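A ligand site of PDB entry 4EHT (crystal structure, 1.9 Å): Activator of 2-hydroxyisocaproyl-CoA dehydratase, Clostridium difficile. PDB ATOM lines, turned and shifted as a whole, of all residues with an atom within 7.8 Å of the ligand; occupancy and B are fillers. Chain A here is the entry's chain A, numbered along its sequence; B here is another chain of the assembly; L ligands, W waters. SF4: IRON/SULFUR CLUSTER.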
ATOM      1  N   ASN A 122     -19.553  18.262 -31.905  1.00  0.00           N
ATOM      2  CA  ASN A 122     -19.288  19.563 -31.299  1.00  0.00           C
ATOM      3  C   ASN A 122     -18.738  19.305 -29.927  1.00  0.00           C
ATOM      4  O   ASN A 122     -19.435  18.758 -29.082  1.00  0.00           O
ATOM      5  CB  ASN A 122     -20.550  20.434 -31.103  1.00  0.00           C
ATOM      6  CG  ASN A 122     -20.328  21.528 -30.034  1.00  0.00           C
ATOM      7  OD1 ASN A 122     -19.237  22.071 -29.928  1.00  0.00           O
ATOM      8  ND2 ASN A 122     -21.353  21.828 -29.228  1.00  0.00           N
ATOM      9  N   LYS A 124     -16.379  21.949 -28.590  1.00  0.00           N
ATOM     10  CA  LYS A 124     -15.714  23.198 -28.190  1.00  0.00           C
ATOM     11  C   LYS A 124     -16.652  24.217 -27.555  1.00  0.00           C
ATOM     12  O   LYS A 124     -16.192  25.191 -26.965  1.00  0.00           O
ATOM     13  CB  LYS A 124     -15.040  23.875 -29.396  1.00  0.00           C
ATOM     14  CG  LYS A 124     -14.088  22.976 -30.164  1.00  0.00           C
ATOM     15  CD  LYS A 124     -13.104  22.304 -29.229  1.00  0.00           C
ATOM     16  CE  LYS A 124     -12.171  21.376 -29.986  1.00  0.00           C
ATOM     17  NZ  LYS A 124     -11.394  20.507 -29.055  1.00  0.00           N
ATOM     18  N   CYS A 125     -17.948  24.024 -27.736  1.00  0.00           N
ATOM     19  CA  CYS A 125     -18.931  25.056 -27.417  1.00  0.00           C
ATOM     20  C   CYS A 125     -19.989  24.447 -26.510  1.00  0.00           C
ATOM     21  O   CYS A 125     -20.490  23.362 -26.782  1.00  0.00           O
ATOM     22  CB  CYS A 125     -19.548  25.587 -28.711  1.00  0.00           C
ATOM     23  SG  CYS A 125     -21.140  26.534 -28.552  1.00  0.00           S
ATOM     24  N   ALA A 126     -20.328  25.123 -25.420  1.00  0.00           N
ATOM     25  CA  ALA A 126     -21.264  24.542 -24.451  1.00  0.00           C
ATOM     26  C   ALA A 126     -22.699  24.515 -24.979  1.00  0.00           C
ATOM     27  O   ALA A 126     -23.509  23.755 -24.445  1.00  0.00           O
ATOM     28  CB  ALA A 126     -21.221  25.276 -23.169  1.00  0.00           C
ATOM     29  N   ALA A 127     -23.028  25.338 -25.984  1.00  0.00           N
ATOM     30  CA  ALA A 127     -24.377  25.271 -26.593  1.00  0.00           C
ATOM     31  C   ALA A 127     -24.620  23.896 -27.228  1.00  0.00           C
ATOM     32  O   ALA A 127     -23.703  23.271 -27.758  1.00  0.00           O
ATOM     33  CB  ALA A 127     -24.546  26.361 -27.638  1.00  0.00           C
ATOM     34  N   GLY A 128     -25.860  23.419 -27.192  1.00  0.00           N
ATOM     35  CA  GLY A 128     -26.190  22.160 -27.831  1.00  0.00           C
ATOM     36  C   GLY A 128     -25.626  20.974 -27.071  1.00  0.00           C
ATOM     37  O   GLY A 128     -25.380  19.951 -27.663  1.00  0.00           O
ATOM     38  N   PHE A 132     -25.466  23.398 -21.413  1.00  0.00           N
ATOM     39  CA  PHE A 132     -26.440  24.455 -21.715  1.00  0.00           C
ATOM     40  C   PHE A 132     -27.714  24.246 -20.885  1.00  0.00           C
ATOM     41  O   PHE A 132     -28.294  25.193 -20.319  1.00  0.00           O
ATOM     42  CB  PHE A 132     -26.766  24.389 -23.210  1.00  0.00           C
ATOM     43  CG  PHE A 132     -27.783  25.414 -23.683  1.00  0.00           C
ATOM     44  CD1 PHE A 132     -29.144  25.102 -23.712  1.00  0.00           C
ATOM     45  CD2 PHE A 132     -27.366  26.657 -24.170  1.00  0.00           C
ATOM     46  CE1 PHE A 132     -30.077  26.040 -24.186  1.00  0.00           C
ATOM     47  CE2 PHE A 132     -28.285  27.596 -24.643  1.00  0.00           C
ATOM     48  CZ  PHE A 132     -29.649  27.298 -24.646  1.00  0.00           C
ATOM     49  N   THR A 163     -27.501  31.973 -30.233  1.00  0.00           N
ATOM     50  CA  THR A 163     -27.025  30.582 -30.214  1.00  0.00           C
ATOM     51  C   THR A 163     -26.043  30.316 -29.045  1.00  0.00           C
ATOM     52  O   THR A 163     -25.841  29.164 -28.662  1.00  0.00           O
ATOM     53  CB  THR A 163     -26.323  30.202 -31.542  1.00  0.00           C
ATOM     54  OG1 THR A 163     -25.373  31.218 -31.878  1.00  0.00           O
ATOM     55  CG2 THR A 163     -27.327  30.065 -32.681  1.00  0.00           C
ATOM     56  N   CYS A 164     -25.443  31.372 -28.501  1.00  0.00           N
ATOM     57  CA  CYS A 164     -24.446  31.265 -27.422  1.00  0.00           C
ATOM     58  C   CYS A 164     -25.103  31.011 -26.070  1.00  0.00           C
ATOM     59  O   CYS A 164     -26.055  31.684 -25.724  1.00  0.00           O
ATOM     60  CB  CYS A 164     -23.646  32.583 -27.318  1.00  0.00           C
ATOM     61  SG  CYS A 164     -22.490  32.654 -25.905  1.00  0.00           S
ATOM     62  N   THR A 165     -24.565  30.069 -25.302  1.00  0.00           N
ATOM     63  CA  THR A 165     -25.109  29.756 -23.982  1.00  0.00           C
ATOM     64  C   THR A 165     -25.179  31.023 -23.101  1.00  0.00           C
ATOM     65  O   THR A 165     -26.172  31.266 -22.405  1.00  0.00           O
ATOM     66  CB  THR A 165     -24.255  28.685 -23.248  1.00  0.00           C
ATOM     67  OG1 THR A 165     -24.132  27.505 -24.061  1.00  0.00           O
ATOM     68  CG2 THR A 165     -24.889  28.320 -21.904  1.00  0.00           C
ATOM     69  N   VAL A 166     -24.121  31.827 -23.120  1.00  0.00           N
ATOM     70  CA  VAL A 166     -24.061  33.003 -22.279  1.00  0.00           C
ATOM     71  C   VAL A 166     -25.105  34.047 -22.692  1.00  0.00           C
ATOM     72  O   VAL A 166     -25.827  34.563 -21.863  1.00  0.00           O
ATOM     73  CB  VAL A 166     -22.645  33.642 -22.264  1.00  0.00           C
ATOM     74  CG1 VAL A 166     -22.604  34.812 -21.337  1.00  0.00           C
ATOM     75  CG2 VAL A 166     -21.585  32.569 -21.845  1.00  0.00           C
ATOM     76  N   PHE A 167     -25.193  34.337 -23.977  1.00  0.00           N
ATOM     77  CA  PHE A 167     -26.154  35.349 -24.429  1.00  0.00           C
ATOM     78  C   PHE A 167     -27.592  34.861 -24.269  1.00  0.00           C
ATOM     79  O   PHE A 167     -28.459  35.623 -23.910  1.00  0.00           O
ATOM     80  CB  PHE A 167     -25.879  35.766 -25.874  1.00  0.00           C
ATOM     81  CG  PHE A 167     -24.555  36.485 -26.067  1.00  0.00           C
ATOM     82  CD1 PHE A 167     -24.061  37.353 -25.105  1.00  0.00           C
ATOM     83  CD2 PHE A 167     -23.792  36.264 -27.202  1.00  0.00           C
ATOM     84  CE1 PHE A 167     -22.812  38.011 -25.272  1.00  0.00           C
ATOM     85  CE2 PHE A 167     -22.549  36.928 -27.392  1.00  0.00           C
ATOM     86  CZ  PHE A 167     -22.063  37.797 -26.423  1.00  0.00           C
ATOM     87  N   ALA A 168     -27.810  33.583 -24.530  1.00  0.00           N
ATOM     88  CA  ALA A 168     -29.124  32.951 -24.365  1.00  0.00           C
ATOM     89  C   ALA A 168     -29.577  33.022 -22.916  1.00  0.00           C
ATOM     90  O   ALA A 168     -30.746  33.222 -22.636  1.00  0.00           O
ATOM     91  CB  ALA A 168     -29.080  31.488 -24.842  1.00  0.00           C
ATOM     92  N   ARG A 196     -29.092  23.177 -32.725  1.00  0.00           N
ATOM     93  CA  ARG A 196     -27.646  23.015 -32.825  1.00  0.00           C
ATOM     94  C   ARG A 196     -27.232  21.561 -33.088  1.00  0.00           C
ATOM     95  O   ARG A 196     -26.293  21.307 -33.829  1.00  0.00           O
ATOM     96  CB  ARG A 196     -26.953  23.547 -31.582  1.00  0.00           C
ATOM     97  CG  ARG A 196     -25.453  23.411 -31.668  1.00  0.00           C
ATOM     98  CD  ARG A 196     -24.736  24.359 -30.731  1.00  0.00           C
ATOM     99  NE  ARG A 196     -23.309  24.071 -30.732  1.00  0.00           N
ATOM    100  CZ  ARG A 196     -22.425  24.655 -31.547  1.00  0.00           C
ATOM    101  NH1 ARG A 196     -22.814  25.578 -32.416  1.00  0.00           N
ATOM    102  NH2 ARG A 196     -21.147  24.317 -31.487  1.00  0.00           N
ATOM    103  N   ASN B 122     -17.144  39.357 -34.712  1.00  0.00           N
ATOM    104  CA  ASN B 122     -17.751  38.299 -33.911  1.00  0.00           C
ATOM    105  C   ASN B 122     -18.842  38.888 -33.057  1.00  0.00           C
ATOM    106  O   ASN B 122     -18.566  39.637 -32.120  1.00  0.00           O
ATOM    107  CB  ASN B 122     -16.763  37.633 -32.940  1.00  0.00           C
ATOM    108  CG  ASN B 122     -17.495  36.864 -31.837  1.00  0.00           C
ATOM    109  OD1 ASN B 122     -18.496  36.208 -32.104  1.00  0.00           O
ATOM    110  ND2 ASN B 122     -17.020  36.967 -30.589  1.00  0.00           N
ATOM    111  N   LYS B 124     -21.600  36.539 -32.259  1.00  0.00           N
ATOM    112  CA  LYS B 124     -22.384  35.333 -31.957  1.00  0.00           C
ATOM    113  C   LYS B 124     -21.887  34.567 -30.748  1.00  0.00           C
ATOM    114  O   LYS B 124     -22.596  33.707 -30.239  1.00  0.00           O
ATOM    115  CB  LYS B 124     -22.353  34.367 -33.144  1.00  0.00           C
ATOM    116  CG  LYS B 124     -23.018  34.869 -34.415  1.00  0.00           C
ATOM    117  CD  LYS B 124     -24.295  35.637 -34.102  1.00  0.00           C
ATOM    118  CE  LYS B 124     -25.068  35.967 -35.389  1.00  0.00           C
ATOM    119  NZ  LYS B 124     -24.227  36.719 -36.394  1.00  0.00           N
ATOM    120  N   CYS B 125     -20.664  34.850 -30.307  1.00  0.00           N
ATOM    121  CA  CYS B 125     -20.018  34.042 -29.273  1.00  0.00           C
ATOM    122  C   CYS B 125     -19.510  35.003 -28.196  1.00  0.00           C
ATOM    123  O   CYS B 125     -18.867  36.006 -28.503  1.00  0.00           O
ATOM    124  CB  CYS B 125     -18.868  33.232 -29.898  1.00  0.00           C
ATOM    125  SG  CYS B 125     -17.703  32.499 -28.730  1.00  0.00           S
ATOM    126  N   ALA B 126     -19.796  34.706 -26.931  1.00  0.00           N
ATOM    127  CA  ALA B 126     -19.396  35.579 -25.847  1.00  0.00           C
ATOM    128  C   ALA B 126     -17.864  35.621 -25.622  1.00  0.00           C
ATOM    129  O   ALA B 126     -17.353  36.603 -25.066  1.00  0.00           O
ATOM    130  CB  ALA B 126     -20.074  35.198 -24.582  1.00  0.00           C
ATOM    131  N   ALA B 127     -17.159  34.551 -26.000  1.00  0.00           N
ATOM    132  CA  ALA B 127     -15.680  34.556 -25.910  1.00  0.00           C
ATOM    133  C   ALA B 127     -15.123  35.729 -26.734  1.00  0.00           C
ATOM    134  O   ALA B 127     -15.688  36.104 -27.768  1.00  0.00           O
ATOM    135  CB  ALA B 127     -15.077  33.253 -26.428  1.00  0.00           C
ATOM    136  N   GLY B 128     -14.004  36.279 -26.303  1.00  0.00           N
ATOM    137  CA  GLY B 128     -13.349  37.324 -27.077  1.00  0.00           C
ATOM    138  C   GLY B 128     -14.167  38.617 -27.069  1.00  0.00           C
ATOM    139  O   GLY B 128     -14.067  39.419 -27.988  1.00  0.00           O
ATOM    140  N   PHE B 132     -17.102  38.068 -21.742  1.00  0.00           N
ATOM    141  CA  PHE B 132     -16.148  37.088 -21.224  1.00  0.00           C
ATOM    142  C   PHE B 132     -15.465  37.651 -19.979  1.00  0.00           C
ATOM    143  O   PHE B 132     -15.362  36.982 -18.946  1.00  0.00           O
ATOM    144  CB  PHE B 132     -15.117  36.742 -22.295  1.00  0.00           C
ATOM    145  CG  PHE B 132     -14.139  35.649 -21.907  1.00  0.00           C
ATOM    146  CD1 PHE B 132     -12.937  35.972 -21.295  1.00  0.00           C
ATOM    147  CD2 PHE B 132     -14.425  34.319 -22.150  1.00  0.00           C
ATOM    148  CE1 PHE B 132     -12.012  34.970 -20.948  1.00  0.00           C
ATOM    149  CE2 PHE B 132     -13.515  33.309 -21.789  1.00  0.00           C
ATOM    150  CZ  PHE B 132     -12.299  33.649 -21.193  1.00  0.00           C
ATOM    151  N   THR B 163     -11.816  27.412 -25.145  1.00  0.00           N
ATOM    152  CA  THR B 163     -12.088  28.696 -25.793  1.00  0.00           C
ATOM    153  C   THR B 163     -13.498  29.230 -25.443  1.00  0.00           C
ATOM    154  O   THR B 163     -13.757  30.419 -25.527  1.00  0.00           O
ATOM    155  CB  THR B 163     -11.971  28.621 -27.324  1.00  0.00           C
ATOM    156  OG1 THR B 163     -12.719  27.506 -27.804  1.00  0.00           O
ATOM    157  CG2 THR B 163     -10.499  28.478 -27.735  1.00  0.00           C
ATOM    158  N   CYS B 164     -14.370  28.326 -25.011  1.00  0.00           N
ATOM    159  CA  CYS B 164     -15.745  28.650 -24.646  1.00  0.00           C
ATOM    160  C   CYS B 164     -15.811  29.384 -23.322  1.00  0.00           C
ATOM    161  O   CYS B 164     -15.201  28.946 -22.368  1.00  0.00           O
ATOM    162  CB  CYS B 164     -16.548  27.336 -24.492  1.00  0.00           C
ATOM    163  SG  CYS B 164     -18.293  27.635 -23.970  1.00  0.00           S
ATOM    164  N   THR B 165     -16.570  30.478 -23.255  1.00  0.00           N
ATOM    165  CA  THR B 165     -16.724  31.214 -22.003  1.00  0.00           C
ATOM    166  C   THR B 165     -17.177  30.285 -20.866  1.00  0.00           C
ATOM    167  O   THR B 165     -16.710  30.390 -19.720  1.00  0.00           O
ATOM    168  CB  THR B 165     -17.737  32.377 -22.146  1.00  0.00           C
ATOM    169  OG1 THR B 165     -17.308  33.269 -23.199  1.00  0.00           O
ATOM    170  CG2 THR B 165     -17.878  33.175 -20.839  1.00  0.00           C
ATOM    171  N   VAL B 166     -18.109  29.402 -21.169  1.00  0.00           N
ATOM    172  CA  VAL B 166     -18.750  28.598 -20.126  1.00  0.00           C
ATOM    173  C   VAL B 166     -17.767  27.578 -19.556  1.00  0.00           C
ATOM    174  O   VAL B 166     -17.609  27.462 -18.345  1.00  0.00           O
ATOM    175  CB  VAL B 166     -20.000  27.914 -20.695  1.00  0.00           C
ATOM    176  CG1 VAL B 166     -20.653  26.980 -19.638  1.00  0.00           C
ATOM    177  CG2 VAL B 166     -20.996  28.984 -21.210  1.00  0.00           C
ATOM    178  N   PHE B 167     -17.090  26.838 -20.429  1.00  0.00           N
ATOM    179  CA  PHE B 167     -16.088  25.859 -19.980  1.00  0.00           C
ATOM    180  C   PHE B 167     -14.882  26.575 -19.326  1.00  0.00           C
ATOM    181  O   PHE B 167     -14.311  26.085 -18.366  1.00  0.00           O
ATOM    182  CB  PHE B 167     -15.631  24.991 -21.158  1.00  0.00           C
ATOM    183  CG  PHE B 167     -16.732  24.157 -21.770  1.00  0.00           C
ATOM    184  CD1 PHE B 167     -17.692  23.556 -20.964  1.00  0.00           C
ATOM    185  CD2 PHE B 167     -16.808  23.965 -23.145  1.00  0.00           C
ATOM    186  CE1 PHE B 167     -18.723  22.777 -21.515  1.00  0.00           C
ATOM    187  CE2 PHE B 167     -17.837  23.173 -23.708  1.00  0.00           C
ATOM    188  CZ  PHE B 167     -18.785  22.586 -22.890  1.00  0.00           C
ATOM    189  N   ALA B 168     -14.545  27.760 -19.824  1.00  0.00           N
ATOM    190  CA  ALA B 168     -13.444  28.527 -19.251  1.00  0.00           C
ATOM    191  C   ALA B 168     -13.763  28.918 -17.817  1.00  0.00           C
ATOM    192  O   ALA B 168     -12.890  28.875 -16.967  1.00  0.00           O
ATOM    193  CB  ALA B 168     -13.110  29.771 -20.112  1.00  0.00           C
ATOM    194  N   ARG B 196      -8.561  35.057 -29.179  1.00  0.00           N
ATOM    195  CA  ARG B 196      -9.806  35.080 -29.953  1.00  0.00           C
ATOM    196  C   ARG B 196      -9.793  36.253 -30.934  1.00  0.00           C
ATOM    197  O   ARG B 196      -9.967  36.085 -32.134  1.00  0.00           O
ATOM    198  CB  ARG B 196     -11.034  35.244 -29.046  1.00  0.00           C
ATOM    199  CG  ARG B 196     -11.318  34.103 -28.077  1.00  0.00           C
ATOM    200  CD  ARG B 196     -11.697  32.798 -28.784  1.00  0.00           C
ATOM    201  NE  ARG B 196     -10.545  32.185 -29.442  1.00  0.00           N
ATOM    202  CZ  ARG B 196      -9.480  31.721 -28.801  1.00  0.00           C
ATOM    203  NH1 ARG B 196      -8.481  31.202 -29.508  1.00  0.00           N
ATOM    204  NH2 ARG B 196      -9.392  31.786 -27.461  1.00  0.00           N
HETATM  205 FE1  SF4 L   1     -18.800  30.827 -27.668  1.00  0.00          FE
HETATM  206 FE2  SF4 L   1     -20.530  28.550 -27.696  1.00  0.00          FE
HETATM  207 FE3  SF4 L   1     -21.163  30.866 -26.193  1.00  0.00          FE
HETATM  208 FE4  SF4 L   1     -19.169  29.130 -25.418  1.00  0.00          FE
HETATM  209  S1  SF4 L   1     -21.369  28.736 -25.677  1.00  0.00           S
HETATM  210  S2  SF4 L   1     -19.070  31.336 -25.574  1.00  0.00           S
HETATM  211  S3  SF4 L   1     -18.301  28.706 -27.409  1.00  0.00           S
HETATM  212  S4  SF4 L   1     -20.937  30.593 -28.316  1.00  0.00           S
HETATM  213  O   HOH W   1     -15.382  27.536 -28.860  1.00  0.00           O
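Within 4 Å of the ligand: Cys 125 of chain A, Ala 126 of chain A, Ala 127 of chain A, Cys 164 of chain A, Thr 165 of chain A, Cys 125 of chain B, Ala 126 of chain B, Ala 127 of chain B, Cys 164 of chain B and Thr 165 of chain B. The nearest printed residue that does not touch the ligand is Lys 124 of chain B (4.02 Å).
Water W1 lies within hydrogen-bond range of OG1 of Thr 163 of chain B (2.9 Å), O of Lys 124 of chain A (3.1 Å) and S3 of the ligand (3.5 Å).
N of Thr 165 of chain A sits close to S1 of the ligand, at 3.5 Å. OG1 of Thr 165 of chain B sits close to S2 of the ligand (3.5 Å). An iron atom (FE2) of the ligand is bound by the side-chain sulfur of Cys 125 of chain A, at 2.3 Å. N of Ala 127 of chain A lies close to S1 of the ligand (3.8 Å). The side-chain sulfur (SG) of Cys 164 of chain A is bound to an iron atom (FE3) of the ligand (2.2 Å). The backbone NH (N) of Ala 127 of chain B sits close to a sulfur (S2) of the ligand (3.8 Å). A sulfur (S1) of the ligand lies close to the backbone NH of Ala 126 of chain A (3.8 Å). The backbone NH (N) of Thr 165 of chain B sits close to a sulfur (S2) of the ligand, 3.5 Å away. S2 of the ligand lies close to N of Ala 126 of chain B. FE4 of the ligand is bound by SG of Cys 164 of chain B, 2.3 Å away. The side-chain hydroxyl (OG1) of Thr 165 of chain A sits close to a sulfur (S1) of the ligand, 3.4 Å away. The side-chain sulfur of Cys 125 of chain B binds an iron atom (FE1) of the ligand (2.3 Å).
The guanidinium group of Arg 196 of chain A lies within hydrogen-bond range of the backbone carbonyl oxygen of Ala 127 of chain A (3.1 Å). The side-chain sulfur of Cys 164 of chain A lies close to the backbone NH of Val 166 of chain A (3.3 Å). The side-chain sulfur of Cys 164 of chain A lies close to the backbone NH of Phe 167 of chain A. The side-chain amide nitrogen (ND2) of Asn 122 of chain B lies within hydrogen-bond range of the backbone carbonyl oxygen (O) of Cys 125 of chain B (2.9 Å). O of Cys 125 of chain A sits at hydrogen-bond distance from ND2 of Asn 122 of chain A (3.0 Å). The side-chain hydroxyl of Thr 165 of chain B sits at hydrogen-bond distance from the backbone NH of Ala 127 of chain B, 3.1 Å away. The side-chain sulfur (SG) of Cys 164 of chain B sits close to the backbone NH (N) of Val 166 of chain B (3.3 Å). The side-chain sulfur (SG) of Cys 164 of chain A sits close to the backbone NH (N) of Ala 126 of chain B, at 3.5 Å.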
